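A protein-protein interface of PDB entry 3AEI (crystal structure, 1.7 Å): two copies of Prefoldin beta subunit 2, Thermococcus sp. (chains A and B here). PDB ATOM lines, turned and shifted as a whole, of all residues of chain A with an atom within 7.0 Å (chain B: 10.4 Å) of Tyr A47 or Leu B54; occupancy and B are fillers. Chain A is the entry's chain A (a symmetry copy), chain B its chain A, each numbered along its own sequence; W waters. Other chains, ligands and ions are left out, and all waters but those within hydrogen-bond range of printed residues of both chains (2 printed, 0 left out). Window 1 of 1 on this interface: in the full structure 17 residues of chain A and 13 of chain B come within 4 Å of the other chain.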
ATOM      1  N   ILE A  37       9.805 -22.350  -3.394  1.00  0.00           N
ATOM      2  CA  ILE A  37       9.376 -21.222  -2.581  1.00  0.00           C
ATOM      3  C   ILE A  37       8.010 -20.709  -2.986  1.00  0.00           C
ATOM      4  O   ILE A  37       7.256 -20.219  -2.143  1.00  0.00           O
ATOM      5  CB  ILE A  37      10.423 -20.090  -2.700  1.00  0.00           C
ATOM      6  CG1 ILE A  37      11.704 -20.524  -1.976  1.00  0.00           C
ATOM      7  CG2 ILE A  37       9.904 -18.790  -2.095  1.00  0.00           C
ATOM      8  CD1 ILE A  37      12.960 -19.693  -2.417  1.00  0.00           C
ATOM      9  N   ARG A  45      10.610 -21.547   6.023  1.00  0.00           N
ATOM     10  CA  ARG A  45      11.576 -20.545   6.405  1.00  0.00           C
ATOM     11  C   ARG A  45      12.647 -20.554   5.310  1.00  0.00           C
ATOM     12  O   ARG A  45      12.883 -21.579   4.676  1.00  0.00           O
ATOM     13  CB  ARG A  45      12.204 -20.905   7.750  1.00  0.00           C
ATOM     14  CG  ARG A  45      11.227 -20.726   8.932  1.00  0.00           C
ATOM     15  CD  ARG A  45      12.027 -20.816  10.234  1.00  0.00           C
ATOM     16  NE  ARG A  45      11.217 -20.797  11.444  1.00  0.00           N
ATOM     17  CZ  ARG A  45      10.936 -19.706  12.146  1.00  0.00           C
ATOM     18  NH1 ARG A  45      11.397 -18.527  11.757  1.00  0.00           N
ATOM     19  NH2 ARG A  45      10.212 -19.800  13.256  1.00  0.00           N
ATOM     20  N   ILE A  46      13.258 -19.396   5.074  1.00  0.00           N
ATOM     21  CA  ILE A  46      14.312 -19.278   4.071  1.00  0.00           C
ATOM     22  C   ILE A  46      15.476 -18.485   4.684  1.00  0.00           C
ATOM     23  O   ILE A  46      15.280 -17.512   5.437  1.00  0.00           O
ATOM     24  CB  ILE A  46      13.833 -18.517   2.820  1.00  0.00           C
ATOM     25  CG1 ILE A  46      12.583 -19.212   2.221  1.00  0.00           C
ATOM     26  CG2 ILE A  46      14.933 -18.513   1.790  1.00  0.00           C
ATOM     27  CD1 ILE A  46      11.754 -18.259   1.262  1.00  0.00           C
ATOM     28  N   TYR A  47      16.698 -18.925   4.386  1.00  0.00           N
ATOM     29  CA  TYR A  47      17.886 -18.212   4.836  1.00  0.00           C
ATOM     30  C   TYR A  47      18.757 -17.896   3.632  1.00  0.00           C
ATOM     31  O   TYR A  47      18.753 -18.627   2.625  1.00  0.00           O
ATOM     32  CB  TYR A  47      18.725 -19.091   5.808  1.00  0.00           C
ATOM     33  CG  TYR A  47      18.034 -19.286   7.143  1.00  0.00           C
ATOM     34  CD1 TYR A  47      18.287 -18.421   8.216  1.00  0.00           C
ATOM     35  CD2 TYR A  47      17.078 -20.297   7.325  1.00  0.00           C
ATOM     36  CE1 TYR A  47      17.609 -18.560   9.412  1.00  0.00           C
ATOM     37  CE2 TYR A  47      16.407 -20.428   8.536  1.00  0.00           C
ATOM     38  CZ  TYR A  47      16.679 -19.551   9.565  1.00  0.00           C
ATOM     39  OH  TYR A  47      16.012 -19.672  10.784  1.00  0.00           O
ATOM     40  N   ARG A  48      19.499 -16.805   3.718  1.00  0.00           N
ATOM     41  CA  ARG A  48      20.447 -16.465   2.666  1.00  0.00           C
ATOM     42  C   ARG A  48      21.839 -16.500   3.302  1.00  0.00           C
ATOM     43  O   ARG A  48      22.052 -16.042   4.442  1.00  0.00           O
ATOM     44  CB  ARG A  48      20.154 -15.098   2.059  1.00  0.00           C
ATOM     45  CG  ARG A  48      21.237 -14.634   1.042  1.00  0.00           C
ATOM     46  CD  ARG A  48      20.697 -13.486   0.207  1.00  0.00           C
ATOM     47  NE  ARG A  48      21.746 -12.925  -0.624  1.00  0.00           N
ATOM     48  CZ  ARG A  48      21.646 -11.761  -1.256  1.00  0.00           C
ATOM     49  NH1 ARG A  48      20.541 -11.049  -1.142  1.00  0.00           N
ATOM     50  NH2 ARG A  48      22.652 -11.320  -1.995  1.00  0.00           N
ATOM     51  N   ALA A  49      22.781 -17.071   2.555  1.00  0.00           N
ATOM     52  CA  ALA A  49      24.142 -17.219   3.036  1.00  0.00           C
ATOM     53  C   ALA A  49      25.016 -16.043   2.632  1.00  0.00           C
ATOM     54  O   ALA A  49      25.062 -15.684   1.455  1.00  0.00           O
ATOM     55  CB  ALA A  49      24.743 -18.496   2.448  1.00  0.00           C
ATOM     56  N   PHE A  50      25.732 -15.480   3.618  1.00  0.00           N
ATOM     57  CA  PHE A  50      26.666 -14.362   3.403  1.00  0.00           C
ATOM     58  C   PHE A  50      27.937 -14.811   4.098  1.00  0.00           C
ATOM     59  O   PHE A  50      28.043 -14.718   5.313  1.00  0.00           O
ATOM     60  CB  PHE A  50      26.158 -13.067   4.075  1.00  0.00           C
ATOM     61  CG  PHE A  50      24.847 -12.580   3.532  1.00  0.00           C
ATOM     62  CD1 PHE A  50      24.792 -11.809   2.365  1.00  0.00           C
ATOM     63  CD2 PHE A  50      23.654 -12.883   4.201  1.00  0.00           C
ATOM     64  CE1 PHE A  50      23.542 -11.334   1.879  1.00  0.00           C
ATOM     65  CE2 PHE A  50      22.410 -12.410   3.706  1.00  0.00           C
ATOM     66  CZ  PHE A  50      22.365 -11.631   2.544  1.00  0.00           C
ATOM     67  N   LEU A  54      24.209 -17.194   8.032  1.00  0.00           N
ATOM     68  CA  LEU A  54      22.978 -17.533   7.332  1.00  0.00           C
ATOM     69  C   LEU A  54      21.991 -16.554   7.978  1.00  0.00           C
ATOM     70  O   LEU A  54      21.854 -16.526   9.188  1.00  0.00           O
ATOM     71  CB  LEU A  54      22.547 -18.973   7.633  1.00  0.00           C
ATOM     72  CG  LEU A  54      23.159 -20.038   6.734  1.00  0.00           C
ATOM     73  CD1 LEU A  54      22.620 -21.398   7.198  1.00  0.00           C
ATOM     74  CD2 LEU A  54      22.773 -19.809   5.271  1.00  0.00           C
ATOM     75  N   VAL A  55      21.301 -15.760   7.178  1.00  0.00           N
ATOM     76  CA  VAL A  55      20.359 -14.756   7.730  1.00  0.00           C
ATOM     77  C   VAL A  55      18.970 -15.043   7.204  1.00  0.00           C
ATOM     78  O   VAL A  55      18.793 -15.223   6.009  1.00  0.00           O
ATOM     79  CB  VAL A  55      20.760 -13.327   7.269  1.00  0.00           C
ATOM     80  CG1 VAL A  55      19.791 -12.300   7.834  1.00  0.00           C
ATOM     81  CG2 VAL A  55      22.170 -13.038   7.724  1.00  0.00           C
ATOM     82  N   GLU A  56      17.976 -15.059   8.088  1.00  0.00           N
ATOM     83  CA  GLU A  56      16.634 -15.352   7.651  1.00  0.00           C
ATOM     84  C   GLU A  56      16.083 -14.249   6.765  1.00  0.00           C
ATOM     85  O   GLU A  56      16.261 -13.066   7.066  1.00  0.00           O
ATOM     86  CB  GLU A  56      15.746 -15.549   8.866  1.00  0.00           C
ATOM     87  CG  GLU A  56      14.368 -16.076   8.502  1.00  0.00           C
ATOM     88  CD  GLU A  56      13.534 -16.427   9.726  1.00  0.00           C
ATOM     89  OE1 GLU A  56      13.859 -15.977  10.829  1.00  0.00           O
ATOM     90  OE2 GLU A  56      12.542 -17.154   9.594  1.00  0.00           O
ATOM     91  N   ILE A  57      15.444 -14.653   5.674  1.00  0.00           N
ATOM     92  CA  ILE A  57      14.852 -13.696   4.766  1.00  0.00           C
ATOM     93  C   ILE A  57      13.437 -14.128   4.442  1.00  0.00           C
ATOM     94  O   ILE A  57      13.061 -15.267   4.695  1.00  0.00           O
ATOM     95  CB  ILE A  57      15.648 -13.512   3.457  1.00  0.00           C
ATOM     96  CG1 ILE A  57      15.750 -14.802   2.663  1.00  0.00           C
ATOM     97  CG2 ILE A  57      17.043 -12.993   3.764  1.00  0.00           C
ATOM     98  CD1 ILE A  57      16.286 -14.575   1.278  1.00  0.00           C
ATOM     99  N   ALA A  62      13.543 -13.512  -0.996  1.00  0.00           N
ATOM    100  CA  ALA A  62      14.175 -14.655  -1.673  1.00  0.00           C
ATOM    101  C   ALA A  62      13.889 -14.610  -3.164  1.00  0.00           C
ATOM    102  O   ALA A  62      14.780 -14.788  -3.971  1.00  0.00           O
ATOM    103  CB  ALA A  62      13.657 -15.968  -1.080  1.00  0.00           C
ATOM    104  N   ARG B  45      13.847 -29.834  12.060  1.00  0.00           N
ATOM    105  CA  ARG B  45      13.661 -29.010  10.889  1.00  0.00           C
ATOM    106  C   ARG B  45      14.753 -29.434   9.901  1.00  0.00           C
ATOM    107  O   ARG B  45      15.823 -29.880  10.306  1.00  0.00           O
ATOM    108  CB  ARG B  45      13.828 -27.536  11.249  1.00  0.00           C
ATOM    109  CG  ARG B  45      12.652 -26.990  12.087  1.00  0.00           C
ATOM    110  CD  ARG B  45      12.764 -25.464  12.133  1.00  0.00           C
ATOM    111  NE  ARG B  45      11.792 -24.812  13.000  1.00  0.00           N
ATOM    112  CZ  ARG B  45      10.625 -24.326  12.596  1.00  0.00           C
ATOM    113  NH1 ARG B  45      10.269 -24.422  11.323  1.00  0.00           N
ATOM    114  NH2 ARG B  45       9.821 -23.721  13.464  1.00  0.00           N
ATOM    115  N   ILE B  46      14.454 -29.321   8.610  1.00  0.00           N
ATOM    116  CA  ILE B  46      15.415 -29.672   7.568  1.00  0.00           C
ATOM    117  C   ILE B  46      15.415 -28.554   6.515  1.00  0.00           C
ATOM    118  O   ILE B  46      14.363 -27.983   6.166  1.00  0.00           O
ATOM    119  CB  ILE B  46      15.042 -30.987   6.858  1.00  0.00           C
ATOM    120  CG1 ILE B  46      14.917 -32.133   7.894  1.00  0.00           C
ATOM    121  CG2 ILE B  46      16.120 -31.337   5.865  1.00  0.00           C
ATOM    122  CD1 ILE B  46      14.082 -33.364   7.343  1.00  0.00           C
ATOM    123  N   TYR B  47      16.609 -28.214   6.031  1.00  0.00           N
ATOM    124  CA  TYR B  47      16.737 -27.227   4.967  1.00  0.00           C
ATOM    125  C   TYR B  47      17.519 -27.838   3.817  1.00  0.00           C
ATOM    126  O   TYR B  47      18.369 -28.725   4.017  1.00  0.00           O
ATOM    127  CB  TYR B  47      17.522 -25.977   5.460  1.00  0.00           C
ATOM    128  CG  TYR B  47      16.728 -25.160   6.461  1.00  0.00           C
ATOM    129  CD1 TYR B  47      15.925 -24.092   6.040  1.00  0.00           C
ATOM    130  CD2 TYR B  47      16.725 -25.488   7.825  1.00  0.00           C
ATOM    131  CE1 TYR B  47      15.151 -23.390   6.943  1.00  0.00           C
ATOM    132  CE2 TYR B  47      15.945 -24.768   8.724  1.00  0.00           C
ATOM    133  CZ  TYR B  47      15.161 -23.729   8.268  1.00  0.00           C
ATOM    134  OH  TYR B  47      14.374 -23.000   9.160  1.00  0.00           O
ATOM    135  N   ARG B  48      17.234 -27.383   2.608  1.00  0.00           N
ATOM    136  CA  ARG B  48      17.996 -27.826   1.448  1.00  0.00           C
ATOM    137  C   ARG B  48      18.692 -26.585   0.883  1.00  0.00           C
ATOM    138  O   ARG B  48      18.113 -25.483   0.809  1.00  0.00           O
ATOM    139  CB  ARG B  48      17.103 -28.480   0.401  1.00  0.00           C
ATOM    140  CG  ARG B  48      17.857 -28.824  -0.917  1.00  0.00           C
ATOM    141  CD  ARG B  48      17.034 -29.802  -1.738  1.00  0.00           C
ATOM    142  NE  ARG B  48      17.634 -29.998  -3.045  1.00  0.00           N
ATOM    143  CZ  ARG B  48      17.012 -30.583  -4.063  1.00  0.00           C
ATOM    144  NH1 ARG B  48      15.777 -31.022  -3.910  1.00  0.00           N
ATOM    145  NH2 ARG B  48      17.631 -30.722  -5.225  1.00  0.00           N
ATOM    146  N   ALA B  49      19.954 -26.775   0.504  1.00  0.00           N
ATOM    147  CA  ALA B  49      20.761 -25.686  -0.012  1.00  0.00           C
ATOM    148  C   ALA B  49      20.680 -25.591  -1.528  1.00  0.00           C
ATOM    149  O   ALA B  49      20.890 -26.587  -2.221  1.00  0.00           O
ATOM    150  CB  ALA B  49      22.220 -25.917   0.382  1.00  0.00           C
ATOM    151  N   PHE B  50      20.411 -24.374  -2.024  1.00  0.00           N
ATOM    152  CA  PHE B  50      20.340 -24.083  -3.466  1.00  0.00           C
ATOM    153  C   PHE B  50      21.216 -22.857  -3.635  1.00  0.00           C
ATOM    154  O   PHE B  50      20.786 -21.748  -3.352  1.00  0.00           O
ATOM    155  CB  PHE B  50      18.900 -23.734  -3.900  1.00  0.00           C
ATOM    156  CG  PHE B  50      17.918 -24.849  -3.684  1.00  0.00           C
ATOM    157  CD1 PHE B  50      17.781 -25.881  -4.620  1.00  0.00           C
ATOM    158  CD2 PHE B  50      17.110 -24.861  -2.540  1.00  0.00           C
ATOM    159  CE1 PHE B  50      16.828 -26.915  -4.411  1.00  0.00           C
ATOM    160  CE2 PHE B  50      16.164 -25.901  -2.336  1.00  0.00           C
ATOM    161  CZ  PHE B  50      16.028 -26.923  -3.282  1.00  0.00           C
ATOM    162  N   SER B  51      22.431 -23.063  -4.114  1.00  0.00           N
ATOM    163  CA  SER B  51      23.383 -21.966  -4.248  1.00  0.00           C
ATOM    164  C   SER B  51      23.470 -21.274  -2.877  1.00  0.00           C
ATOM    165  O   SER B  51      23.803 -21.920  -1.874  1.00  0.00           O
ATOM    166  CB  SER B  51      22.965 -20.983  -5.353  1.00  0.00           C
ATOM    167  OG  SER B  51      24.007 -20.002  -5.532  1.00  0.00           O
ATOM    168  N   ASP B  52      23.177 -19.984  -2.818  1.00  0.00           N
ATOM    169  CA  ASP B  52      23.281 -19.290  -1.550  1.00  0.00           C
ATOM    170  C   ASP B  52      22.010 -19.151  -0.720  1.00  0.00           C
ATOM    171  O   ASP B  52      21.949 -18.303   0.173  1.00  0.00           O
ATOM    172  CB  ASP B  52      23.957 -17.920  -1.759  1.00  0.00           C
ATOM    173  CG  ASP B  52      23.155 -16.971  -2.642  1.00  0.00           C
ATOM    174  OD1 ASP B  52      22.188 -17.412  -3.259  1.00  0.00           O
ATOM    175  OD2 ASP B  52      23.502 -15.764  -2.728  1.00  0.00           O
ATOM    176  N   LEU B  53      21.017 -19.992  -1.012  1.00  0.00           N
ATOM    177  CA  LEU B  53      19.781 -19.981  -0.240  1.00  0.00           C
ATOM    178  C   LEU B  53      19.612 -21.321   0.453  1.00  0.00           C
ATOM    179  O   LEU B  53      20.076 -22.318  -0.041  1.00  0.00           O
ATOM    180  CB  LEU B  53      18.567 -19.758  -1.131  1.00  0.00           C
ATOM    181  CG  LEU B  53      18.494 -18.389  -1.779  1.00  0.00           C
ATOM    182  CD1 LEU B  53      17.218 -18.371  -2.649  1.00  0.00           C
ATOM    183  CD2 LEU B  53      18.388 -17.295  -0.713  1.00  0.00           C
ATOM    184  N   LEU B  54      18.998 -21.311   1.632  1.00  0.00           N
ATOM    185  CA  LEU B  54      18.679 -22.532   2.358  1.00  0.00           C
ATOM    186  C   LEU B  54      17.150 -22.446   2.427  1.00  0.00           C
ATOM    187  O   LEU B  54      16.610 -21.461   2.898  1.00  0.00           O
ATOM    188  CB  LEU B  54      19.262 -22.500   3.777  1.00  0.00           C
ATOM    189  CG  LEU B  54      20.696 -22.993   3.902  1.00  0.00           C
ATOM    190  CD1 LEU B  54      21.097 -22.873   5.379  1.00  0.00           C
ATOM    191  CD2 LEU B  54      20.817 -24.453   3.458  1.00  0.00           C
ATOM    192  N   VAL B  55      16.457 -23.472   1.968  1.00  0.00           N
ATOM    193  CA  VAL B  55      14.974 -23.446   1.960  1.00  0.00           C
ATOM    194  C   VAL B  55      14.456 -24.594   2.800  1.00  0.00           C
ATOM    195  O   VAL B  55      14.892 -25.723   2.629  1.00  0.00           O
ATOM    196  CB  VAL B  55      14.437 -23.632   0.513  1.00  0.00           C
ATOM    197  CG1 VAL B  55      12.916 -23.606   0.510  1.00  0.00           C
ATOM    198  CG2 VAL B  55      14.991 -22.534  -0.364  1.00  0.00           C
ATOM    199  N   GLU B  56      13.508 -24.316   3.689  1.00  0.00           N
ATOM    200  CA  GLU B  56      12.993 -25.363   4.537  1.00  0.00           C
ATOM    201  C   GLU B  56      12.212 -26.391   3.739  1.00  0.00           C
ATOM    202  O   GLU B  56      11.422 -26.029   2.863  1.00  0.00           O
ATOM    203  CB  GLU B  56      12.115 -24.749   5.612  1.00  0.00           C
ATOM    204  CG  GLU B  56      11.709 -25.754   6.677  1.00  0.00           C
ATOM    205  CD  GLU B  56      10.966 -25.106   7.838  1.00  0.00           C
ATOM    206  OE1 GLU B  56      10.479 -23.980   7.693  1.00  0.00           O
ATOM    207  OE2 GLU B  56      10.861 -25.721   8.907  1.00  0.00           O
ATOM    208  N   ILE B  57      12.461 -27.662   4.038  1.00  0.00           N
ATOM    209  CA  ILE B  57      11.760 -28.732   3.364  1.00  0.00           C
ATOM    210  C   ILE B  57      11.251 -29.718   4.394  1.00  0.00           C
ATOM    211  O   ILE B  57      11.683 -29.698   5.541  1.00  0.00           O
ATOM    212  CB  ILE B  57      12.620 -29.473   2.319  1.00  0.00           C
ATOM    213  CG1 ILE B  57      13.839 -30.129   2.944  1.00  0.00           C
ATOM    214  CG2 ILE B  57      13.063 -28.510   1.230  1.00  0.00           C
ATOM    215  CD1 ILE B  57      14.529 -31.066   1.993  1.00  0.00           C
HETATM  216  O   HOH W   1      10.535 -21.703  15.422  1.00  0.00           O
HETATM  217  O   HOH W   2      24.347 -14.320  -0.692  1.00  0.00           O
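The side-chain carboxylate of Asp B52 lies within salt-bridge range of the guanidinium group of Arg A48 (3.9 Å).
The backbone NH (N) of Ala A49 sits at hydrogen-bond distance from the backbone carbonyl oxygen (O) of Asp B52 (2.8 Å).
The backbone carbonyl oxygen of Tyr A47 sits at hydrogen-bond distance from the backbone NH of Leu B54, 2.9 Å away.
The side-chain carboxylate (OE1) of Glu B56 lies within hydrogen-bond range of the backbone NH (N) of Arg A45, at 3.0 Å.
The guanidinium group (NH1) of Arg B45 is in salt-bridge range of the side-chain carboxylate (OE2) of Glu B56 (2.8 Å).
The backbone carbonyl oxygen (O) of Arg B48 lies within hydrogen-bond range of the backbone NH (N) of Val B55 (2.9 Å).
The side-chain carboxylate (OE2) of Glu A56 is in salt-bridge range of the guanidinium group (NH1) of Arg A45 (2.8 Å).
The backbone NH (N) of Ile A57 is in hydrogen-bond range of the backbone carbonyl oxygen (O) of Ile A46, 2.9 Å away.
The backbone carbonyl oxygen (O) of Arg A48 lies within hydrogen-bond range of the backbone NH (N) of Val A55, 2.9 Å away.
Arg A45 touches Arg B45.
Arg A45 touches Tyr B47.
Arg A45 touches Val B55.
Ile A46 touches Leu B54.
Tyr B47 touches Tyr A47 (OH to CE2, 3.3 Å).
O of Tyr A47 touches CA of Leu B53, 3.3 Å away.
Leu B53 touches Arg A48.
CD1 of Leu A54 touches CD1 of Leu B54 (2.8 Å).
CD1 of Ile A57 touches CD2 of Leu B53 (3.97 Å).
Ile A37 touches none of the printed residues of chain B.
Ile A46 touches just one residue of chain B: Leu B54 (3.4 Å).
Of chain B, only Tyr B47, Leu B53 and Leu B54 come within 4 Å of Tyr A47.
Of the printed residues of chain B, Arg A48 touches Asp B52 and Leu B53.
Of the printed residues of chain B, Ala A49 touches Asp B52.
Glu A56 touches none of the printed residues of chain B.
Ile A57 touches one residue of chain B.
Of the printed residues of chain A, Asp B52 touches Arg A48 and Ala A49.
Printed residues of chain A within 4 Å of Leu B53: Tyr A47, Arg A48 and Ile A57.
Leu B54 touches just these residues of chain A: Ile A46 (3.4 Å), Tyr A47 (2.9 Å) and Leu A54 (2.8 Å).
Of the printed residues of chain A, Glu B56 touches Arg A45.
The nearest residue of chain B that does not touch Tyr A47 is Asp B52 (4.04 Å).
The nearest printed residue of chain B that does not touch Ala A49 is Leu B53 (4.9 Å).
Of the 13 printed residues of chain B, 7 touch a printed residue of chain A.
Of the 12 printed residues of chain A, 7 touch a printed residue of chain B.
Hydrophobic or aromatic side chains of chain A that line the printed part of chain B: Ile A46, Tyr A47, Ala A49, Leu A54 and Ile A57.
Arg A45 touches Tyr B47, but with the chains exchanged Tyr A47 does not touch Arg B45 (6.8 Å).
Arg A45 touches Val B55, but with the chains exchanged Val A55 does not touch Arg B45 (13.1 Å).
Ile A46 touches Leu B54, but with the chains exchanged Leu A54 does not touch Ile B46 (10.2 Å).
Leu A54 touches its own counterpart, Leu B54.
10 positions are printed for both chains.
Water W2 lies within hydrogen-bond range of the side-chain carboxylate of Asp B52 (2.6 Å), the backbone carbonyl oxygen of Ala A49 (2.6 Å) and the guanidinium group of Arg A48 (3.0 Å).
Water W1 bridges NH2 of Arg B45 (2.9 Å) and NH2 of Arg A45 (2.9 Å).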
